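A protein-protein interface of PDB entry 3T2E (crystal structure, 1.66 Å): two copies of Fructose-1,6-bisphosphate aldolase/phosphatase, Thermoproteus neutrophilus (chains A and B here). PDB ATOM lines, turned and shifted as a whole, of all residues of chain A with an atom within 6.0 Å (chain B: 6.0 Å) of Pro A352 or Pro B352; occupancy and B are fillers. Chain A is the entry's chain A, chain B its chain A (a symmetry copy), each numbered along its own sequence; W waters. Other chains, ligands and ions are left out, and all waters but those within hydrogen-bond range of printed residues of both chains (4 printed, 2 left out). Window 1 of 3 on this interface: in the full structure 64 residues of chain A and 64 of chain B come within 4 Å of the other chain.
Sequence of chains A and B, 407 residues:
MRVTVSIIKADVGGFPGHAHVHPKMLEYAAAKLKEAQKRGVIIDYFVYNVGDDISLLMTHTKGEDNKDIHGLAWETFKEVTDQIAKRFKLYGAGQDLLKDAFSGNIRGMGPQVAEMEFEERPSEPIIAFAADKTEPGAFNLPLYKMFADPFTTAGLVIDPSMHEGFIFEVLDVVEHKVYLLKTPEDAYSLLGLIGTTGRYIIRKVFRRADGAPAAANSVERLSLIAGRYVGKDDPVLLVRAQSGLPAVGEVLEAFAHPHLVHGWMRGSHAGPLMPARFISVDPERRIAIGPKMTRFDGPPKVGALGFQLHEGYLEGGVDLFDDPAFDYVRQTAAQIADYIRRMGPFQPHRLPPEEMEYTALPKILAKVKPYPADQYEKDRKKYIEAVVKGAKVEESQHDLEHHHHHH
Thr A196 touches Gln B347, and with the chains exchanged Gln A347 touches Thr B196.
Thr A196 touches Arg B350, and with the chains exchanged Arg A350 touches Thr B196.
Gln A347 touches Glu B355, and with the chains exchanged Glu A355 touches Gln B347.
Pro B352 touches its own counterpart, Pro A352.
10 positions are printed for both chains.
Of the 12 pairs that touch across the chains among the printed residues, 12 have their exchanged pair printed and touching as well.
The side-chain hydroxyl (OG1) of Thr A196 lies within hydrogen-bond range of the guanidinium group (NH1) of Arg B350, at 2.9 Å.
The side-chain amide nitrogen of Gln A347 sits at hydrogen-bond distance from the side-chain carboxylate of Glu B355 (3.0 Å).
The guanidinium group of Arg A350 lies within hydrogen-bond range of the side-chain hydroxyl of Thr B196.
OE2 of Glu A355 is in hydrogen-bond range of NE2 of Gln B347 (3.0 Å).
The side-chain carboxylate (OE1) of Glu B354 lies close to the side-chain carboxylate (OE1) of Glu A354 (2.4 Å).
Among the printed residues, merely in contact across the chains: Thr A196 with Gln B347, Thr A196 with Pro B353, His A262 with Gln B347, Gln A347 with Thr B196, Gln A347 with His B262, Pro A352 with Pro B352 and Pro A353 with Thr B196.
Of the 10 printed residues of chain A, 8 touch a printed residue of chain B.
Printed residues of chain A that touch a printed residue of chain B: Thr A196, His A262, Gln A347, Arg A350, Pro A352, Pro A353, Glu A354 and Glu A355.
Hydrophobic or aromatic side chains of chain A within 4 Å of the printed part of chain B: His A262, Pro A352 and Pro A353.
Of the 10 printed residues of chain B, 8 touch a printed residue of chain A.
Hydrophobic or aromatic side chains of chain B within 4 Å of the printed part of chain A: His B262, Pro B352 and Pro B353.
OE1 of Glu A355 is in hydrogen-bond range of ND1 of His A262, 3.5 Å away.
NH1 of Arg A350 sits at hydrogen-bond distance from OE1 of Gln A347 (3.5 Å).
NE of Arg A350 sits close to SD of Met A356.
A ring nitrogen (ND1) of His B262 lies within hydrogen-bond range of the side-chain carboxylate (OE1) of Glu B355 (3.5 Å).
OE1 of Gln B347 sits at hydrogen-bond distance from NH1 of Arg B350.
NE of Arg B350 sits close to SD of Met B356 (3.6 Å).
Of the printed residues of chain B, Arg A350 touches Thr B196 (2.9 Å).
Leu A351 touches none of the printed residues of chain B.
Pro A352 touches just one residue of chain B: Pro B352.
Printed residues of chain B within 4 Å of Glu A355: Gln B347 (3.0 Å).
Of chain A, only Pro A352 comes within 4 Å of Pro B352.
Of the printed residues of chain A, Glu B355 touches Gln A347.
Water W4 bridges the side-chain amide oxygen of Gln B347 (2.7 Å) and the side-chain carboxylate of Glu A355 (2.7 Å).
Water W2 lies within hydrogen-bond range of the side-chain amide oxygen (OE1) of Gln A347 and the side-chain carboxylate (OE1) of Glu B355.
Water W1 lies within hydrogen-bond range of a ring nitrogen (NE2) of His A262 and the side-chain amide nitrogen (NE2) of Gln B347.
Water W3 lies within hydrogen-bond range of NE2 of His B262 (2.8 Å) and NE2 of Gln A347 (2.9 Å).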
ATOM      1  N   THR A 196      13.656 -32.855  -6.732  1.00  0.00           N
ATOM      2  CA  THR A 196      14.132 -31.494  -6.436  1.00  0.00           C
ATOM      3  C   THR A 196      13.694 -30.678  -7.639  1.00  0.00           C
ATOM      4  O   THR A 196      14.425 -30.451  -8.656  1.00  0.00           O
ATOM      5  CB  THR A 196      15.661 -31.521  -6.356  1.00  0.00           C
ATOM      6  OG1 THR A 196      16.007 -32.411  -5.309  1.00  0.00           O
ATOM      7  CG2 THR A 196      16.183 -30.097  -6.056  1.00  0.00           C
ATOM      8  N   HIS A 262       5.687 -25.187  -6.661  1.00  0.00           N
ATOM      9  CA  HIS A 262       6.303 -23.897  -6.269  1.00  0.00           C
ATOM     10  C   HIS A 262       5.919 -22.759  -7.151  1.00  0.00           C
ATOM     11  O   HIS A 262       5.914 -22.947  -8.403  1.00  0.00           O
ATOM     12  CB  HIS A 262       7.839 -24.030  -6.346  1.00  0.00           C
ATOM     13  CG  HIS A 262       8.383 -25.013  -5.376  1.00  0.00           C
ATOM     14  ND1 HIS A 262       9.747 -25.294  -5.342  1.00  0.00           N
ATOM     15  CD2 HIS A 262       7.822 -25.721  -4.347  1.00  0.00           C
ATOM     16  CE1 HIS A 262       9.981 -26.159  -4.362  1.00  0.00           C
ATOM     17  NE2 HIS A 262       8.844 -26.443  -3.753  1.00  0.00           N
ATOM     18  N   GLN A 347       7.871 -21.448   5.923  1.00  0.00           N
ATOM     19  CA  GLN A 347       8.152 -22.727   5.220  1.00  0.00           C
ATOM     20  C   GLN A 347       7.326 -23.818   5.888  1.00  0.00           C
ATOM     21  O   GLN A 347       7.178 -23.807   7.117  1.00  0.00           O
ATOM     22  CB  GLN A 347       9.647 -23.234   5.292  1.00  0.00           C
ATOM     23  CG  GLN A 347      10.524 -22.379   4.435  1.00  0.00           C
ATOM     24  CD  GLN A 347      11.916 -23.008   4.401  1.00  0.00           C
ATOM     25  OE1 GLN A 347      12.727 -22.429   5.020  1.00  0.00           O
ATOM     26  NE2 GLN A 347      12.163 -24.163   3.737  1.00  0.00           N
ATOM     27  N   ARG A 350       5.773 -20.923   2.501  1.00  0.00           N
ATOM     28  CA  ARG A 350       6.801 -20.055   1.844  1.00  0.00           C
ATOM     29  C   ARG A 350       7.929 -20.936   1.438  1.00  0.00           C
ATOM     30  O   ARG A 350       8.222 -21.960   2.080  1.00  0.00           O
ATOM     31  CB  ARG A 350       7.334 -19.041   2.920  1.00  0.00           C
ATOM     32  CG  ARG A 350       7.950 -17.781   2.296  1.00  0.00           C
ATOM     33  CD  ARG A 350       9.135 -17.340   3.209  1.00  0.00           C
ATOM     34  NE  ARG A 350      10.256 -18.283   3.085  1.00  0.00           N
ATOM     35  CZ  ARG A 350      11.337 -18.330   3.889  1.00  0.00           C
ATOM     36  NH1 ARG A 350      12.296 -19.256   3.658  1.00  0.00           N
ATOM     37  NH2 ARG A 350      11.389 -17.451   4.912  1.00  0.00           N
ATOM     38  N   LEU A 351       8.553 -20.586   0.279  1.00  0.00           N
ATOM     39  CA  LEU A 351       9.603 -21.472  -0.254  1.00  0.00           C
ATOM     40  C   LEU A 351      10.950 -21.376   0.489  1.00  0.00           C
ATOM     41  O   LEU A 351      11.159 -20.428   1.264  1.00  0.00           O
ATOM     42  CB  LEU A 351       9.825 -21.134  -1.736  1.00  0.00           C
ATOM     43  CG  LEU A 351       8.595 -21.555  -2.596  1.00  0.00           C
ATOM     44  CD1 LEU A 351       8.987 -21.114  -4.046  1.00  0.00           C
ATOM     45  CD2 LEU A 351       8.244 -23.027  -2.470  1.00  0.00           C
ATOM     46  N   PRO A 352      11.850 -22.332   0.257  1.00  0.00           N
ATOM     47  CA  PRO A 352      13.166 -22.291   0.894  1.00  0.00           C
ATOM     48  C   PRO A 352      13.879 -20.971   0.428  1.00  0.00           C
ATOM     49  O   PRO A 352      13.584 -20.361  -0.568  1.00  0.00           O
ATOM     50  CB  PRO A 352      13.846 -23.555   0.327  1.00  0.00           C
ATOM     51  CG  PRO A 352      12.750 -24.443  -0.117  1.00  0.00           C
ATOM     52  CD  PRO A 352      11.671 -23.531  -0.574  1.00  0.00           C
ATOM     53  N   PRO A 353      14.822 -20.501   1.212  1.00  0.00           N
ATOM     54  CA  PRO A 353      15.292 -19.165   0.974  1.00  0.00           C
ATOM     55  C   PRO A 353      16.091 -19.066  -0.396  1.00  0.00           C
ATOM     56  O   PRO A 353      15.957 -18.079  -1.085  1.00  0.00           O
ATOM     57  CB  PRO A 353      16.183 -18.917   2.218  1.00  0.00           C
ATOM     58  CG  PRO A 353      16.508 -20.263   2.806  1.00  0.00           C
ATOM     59  CD  PRO A 353      15.278 -21.121   2.445  1.00  0.00           C
ATOM     60  N   GLU A 354      16.676 -20.169  -0.854  1.00  0.00           N
ATOM     61  CA  GLU A 354      17.382 -20.158  -2.171  1.00  0.00           C
ATOM     62  C   GLU A 354      16.391 -20.082  -3.294  1.00  0.00           C
ATOM     63  O   GLU A 354      16.760 -19.690  -4.397  1.00  0.00           O
ATOM     64  CB  GLU A 354      18.216 -21.435  -2.420  1.00  0.00           C
ATOM     65  CG  GLU A 354      18.773 -22.128  -1.154  1.00  0.00           C
ATOM     66  CD  GLU A 354      17.575 -22.736  -0.291  1.00  0.00           C
ATOM     67  OE1 GLU A 354      17.134 -23.860  -0.516  1.00  0.00           O
ATOM     68  OE2 GLU A 354      17.064 -22.085   0.572  1.00  0.00           O
ATOM     69  N   GLU A 355      15.129 -20.431  -3.025  1.00  0.00           N
ATOM     70  CA  GLU A 355      14.115 -20.738  -4.065  1.00  0.00           C
ATOM     71  C   GLU A 355      13.080 -19.676  -4.220  1.00  0.00           C
ATOM     72  O   GLU A 355      12.259 -19.698  -5.161  1.00  0.00           O
ATOM     73  CB  GLU A 355      13.407 -22.094  -3.813  1.00  0.00           C
ATOM     74  CG  GLU A 355      14.388 -23.275  -3.719  1.00  0.00           C
ATOM     75  CD  GLU A 355      13.783 -24.714  -3.892  1.00  0.00           C
ATOM     76  OE1 GLU A 355      13.168 -24.941  -4.968  1.00  0.00           O
ATOM     77  OE2 GLU A 355      14.057 -25.640  -3.023  1.00  0.00           O
ATOM     78  N   MET A 356      13.146 -18.652  -3.389  1.00  0.00           N
ATOM     79  CA  MET A 356      12.100 -17.655  -3.478  1.00  0.00           C
ATOM     80  C   MET A 356      12.498 -16.574  -4.425  1.00  0.00           C
ATOM     81  O   MET A 356      13.662 -16.164  -4.454  1.00  0.00           O
ATOM     82  CB  MET A 356      11.962 -17.029  -2.147  1.00  0.00           C
ATOM     83  CG  MET A 356      11.395 -18.010  -1.240  1.00  0.00           C
ATOM     84  SD  MET A 356      10.878 -16.852  -0.176  1.00  0.00           S
ATOM     85  CE  MET A 356      12.379 -16.536   0.791  1.00  0.00           C
ATOM     86  N   THR B 196      12.100 -19.146   7.768  1.00  0.00           N
ATOM     87  CA  THR B 196      13.055 -20.164   7.302  1.00  0.00           C
ATOM     88  C   THR B 196      13.308 -21.025   8.527  1.00  0.00           C
ATOM     89  O   THR B 196      14.269 -20.846   9.343  1.00  0.00           O
ATOM     90  CB  THR B 196      14.350 -19.461   6.886  1.00  0.00           C
ATOM     91  OG1 THR B 196      14.019 -18.567   5.837  1.00  0.00           O
ATOM     92  CG2 THR B 196      15.371 -20.515   6.402  1.00  0.00           C
ATOM     93  N   HIS B 262       8.608 -29.560   9.063  1.00  0.00           N
ATOM     94  CA  HIS B 262       9.631 -30.457   8.476  1.00  0.00           C
ATOM     95  C   HIS B 262      10.003 -31.598   9.359  1.00  0.00           C
ATOM     96  O   HIS B 262      10.193 -31.366  10.589  1.00  0.00           O
ATOM     97  CB  HIS B 262      10.919 -29.648   8.217  1.00  0.00           C
ATOM     98  CG  HIS B 262      10.736 -28.578   7.204  1.00  0.00           C
ATOM     99  ND1 HIS B 262      11.784 -27.719   6.882  1.00  0.00           N
ATOM    100  CD2 HIS B 262       9.705 -28.252   6.364  1.00  0.00           C
ATOM    101  CE1 HIS B 262      11.383 -26.894   5.922  1.00  0.00           C
ATOM    102  NE2 HIS B 262      10.134 -27.181   5.598  1.00  0.00           N
ATOM    103  N   GLN B 347       9.374 -32.592  -3.872  1.00  0.00           N
ATOM    104  CA  GLN B 347       9.201 -31.286  -3.182  1.00  0.00           C
ATOM    105  C   GLN B 347       7.850 -30.718  -3.591  1.00  0.00           C
ATOM    106  O   GLN B 347       7.453 -30.859  -4.755  1.00  0.00           O
ATOM    107  CB  GLN B 347      10.254 -30.170  -3.558  1.00  0.00           C
ATOM    108  CG  GLN B 347      11.586 -30.495  -2.964  1.00  0.00           C
ATOM    109  CD  GLN B 347      12.519 -29.310  -3.207  1.00  0.00           C
ATOM    110  OE1 GLN B 347      13.343 -29.497  -4.021  1.00  0.00           O
ATOM    111  NE2 GLN B 347      12.364 -28.133  -2.554  1.00  0.00           N
ATOM    112  N   ARG B 350       8.551 -33.817  -0.102  1.00  0.00           N
ATOM    113  CA  ARG B 350       9.976 -34.097   0.263  1.00  0.00           C
ATOM    114  C   ARG B 350      10.650 -32.784   0.454  1.00  0.00           C
ATOM    115  O   ARG B 350      10.304 -31.773  -0.182  1.00  0.00           O
ATOM    116  CB  ARG B 350      10.652 -34.821  -0.958  1.00  0.00           C
ATOM    117  CG  ARG B 350      11.888 -35.637  -0.554  1.00  0.00           C
ATOM    118  CD  ARG B 350      12.909 -35.551  -1.730  1.00  0.00           C
ATOM    119  NE  ARG B 350      13.486 -34.200  -1.808  1.00  0.00           N
ATOM    120  CZ  ARG B 350      14.223 -33.718  -2.828  1.00  0.00           C
ATOM    121  NH1 ARG B 350      14.691 -32.450  -2.767  1.00  0.00           N
ATOM    122  NH2 ARG B 350      14.433 -34.534  -3.883  1.00  0.00           N
ATOM    123  N   LEU B 351      11.605 -32.756   1.424  1.00  0.00           N
ATOM    124  CA  LEU B 351      12.237 -31.467   1.758  1.00  0.00           C
ATOM    125  C   LEU B 351      13.282 -30.990   0.730  1.00  0.00           C
ATOM    126  O   LEU B 351      13.714 -31.784  -0.121  1.00  0.00           O
ATOM    127  CB  LEU B 351      12.910 -31.591   3.133  1.00  0.00           C
ATOM    128  CG  LEU B 351      11.847 -31.719   4.265  1.00  0.00           C
ATOM    129  CD1 LEU B 351      12.706 -31.861   5.567  1.00  0.00           C
ATOM    130  CD2 LEU B 351      10.857 -30.568   4.300  1.00  0.00           C
ATOM    131  N   PRO B 352      13.686 -29.722   0.806  1.00  0.00           N
ATOM    132  CA  PRO B 352      14.702 -29.204  -0.109  1.00  0.00           C
ATOM    133  C   PRO B 352      16.014 -30.039   0.116  1.00  0.00           C
ATOM    134  O   PRO B 352      16.253 -30.663   1.119  1.00  0.00           O
ATOM    135  CB  PRO B 352      14.853 -27.742   0.359  1.00  0.00           C
ATOM    136  CG  PRO B 352      13.605 -27.415   1.083  1.00  0.00           C
ATOM    137  CD  PRO B 352      13.179 -28.687   1.718  1.00  0.00           C
ATOM    138  N   PRO B 353      16.867 -30.079  -0.882  1.00  0.00           N
ATOM    139  CA  PRO B 353      17.924 -31.049  -0.826  1.00  0.00           C
ATOM    140  C   PRO B 353      18.966 -30.707   0.325  1.00  0.00           C
ATOM    141  O   PRO B 353      19.444 -31.611   0.973  1.00  0.00           O
ATOM    142  CB  PRO B 353      18.530 -30.938  -2.248  1.00  0.00           C
ATOM    143  CG  PRO B 353      18.079 -29.623  -2.821  1.00  0.00           C
ATOM    144  CD  PRO B 353      16.711 -29.388  -2.151  1.00  0.00           C
ATOM    145  N   GLU B 354      19.080 -29.436   0.699  1.00  0.00           N
ATOM    146  CA  GLU B 354      19.991 -29.061   1.824  1.00  0.00           C
ATOM    147  C   GLU B 354      19.416 -29.512   3.134  1.00  0.00           C
ATOM    148  O   GLU B 354      20.156 -29.638   4.105  1.00  0.00           O
ATOM    149  CB  GLU B 354      20.197 -27.534   1.949  1.00  0.00           C
ATOM    150  CG  GLU B 354      20.089 -26.734   0.630  1.00  0.00           C
ATOM    151  CD  GLU B 354      18.587 -26.772   0.088  1.00  0.00           C
ATOM    152  OE1 GLU B 354      17.753 -25.954   0.465  1.00  0.00           O
ATOM    153  OE2 GLU B 354      18.244 -27.628  -0.674  1.00  0.00           O
ATOM    154  N   GLU B 355      18.106 -29.779   3.171  1.00  0.00           N
ATOM    155  CA  GLU B 355      17.321 -29.902   4.425  1.00  0.00           C
ATOM    156  C   GLU B 355      16.934 -31.305   4.749  1.00  0.00           C
ATOM    157  O   GLU B 355      16.422 -31.602   5.849  1.00  0.00           O
ATOM    158  CB  GLU B 355      16.046 -29.022   4.409  1.00  0.00           C
ATOM    159  CG  GLU B 355      16.347 -27.533   4.163  1.00  0.00           C
ATOM    160  CD  GLU B 355      15.218 -26.509   4.542  1.00  0.00           C
ATOM    161  OE1 GLU B 355      14.823 -26.525   5.738  1.00  0.00           O
ATOM    162  OE2 GLU B 355      14.848 -25.606   3.685  1.00  0.00           O
ATOM    163  N   MET B 356      17.264 -32.234   3.871  1.00  0.00           N
ATOM    164  CA  MET B 356      16.824 -33.587   4.137  1.00  0.00           C
ATOM    165  C   MET B 356      17.862 -34.324   4.913  1.00  0.00           C
ATOM    166  O   MET B 356      19.061 -34.169   4.661  1.00  0.00           O
ATOM    167  CB  MET B 356      16.688 -34.279   2.839  1.00  0.00           C
ATOM    168  CG  MET B 356      15.557 -33.704   2.135  1.00  0.00           C
ATOM    169  SD  MET B 356      15.390 -35.027   1.152  1.00  0.00           S
ATOM    170  CE  MET B 356      16.617 -34.689  -0.140  1.00  0.00           C
HETATM  171  O   HOH W   1      10.019 -26.968  -1.231  1.00  0.00           O
HETATM  172  O   HOH W   2      14.541 -23.890   6.444  1.00  0.00           O
HETATM  173  O   HOH W   3      10.358 -26.322   2.908  1.00  0.00           O
HETATM  174  O   HOH W   4      13.945 -27.458  -5.732  1.00  0.00           O
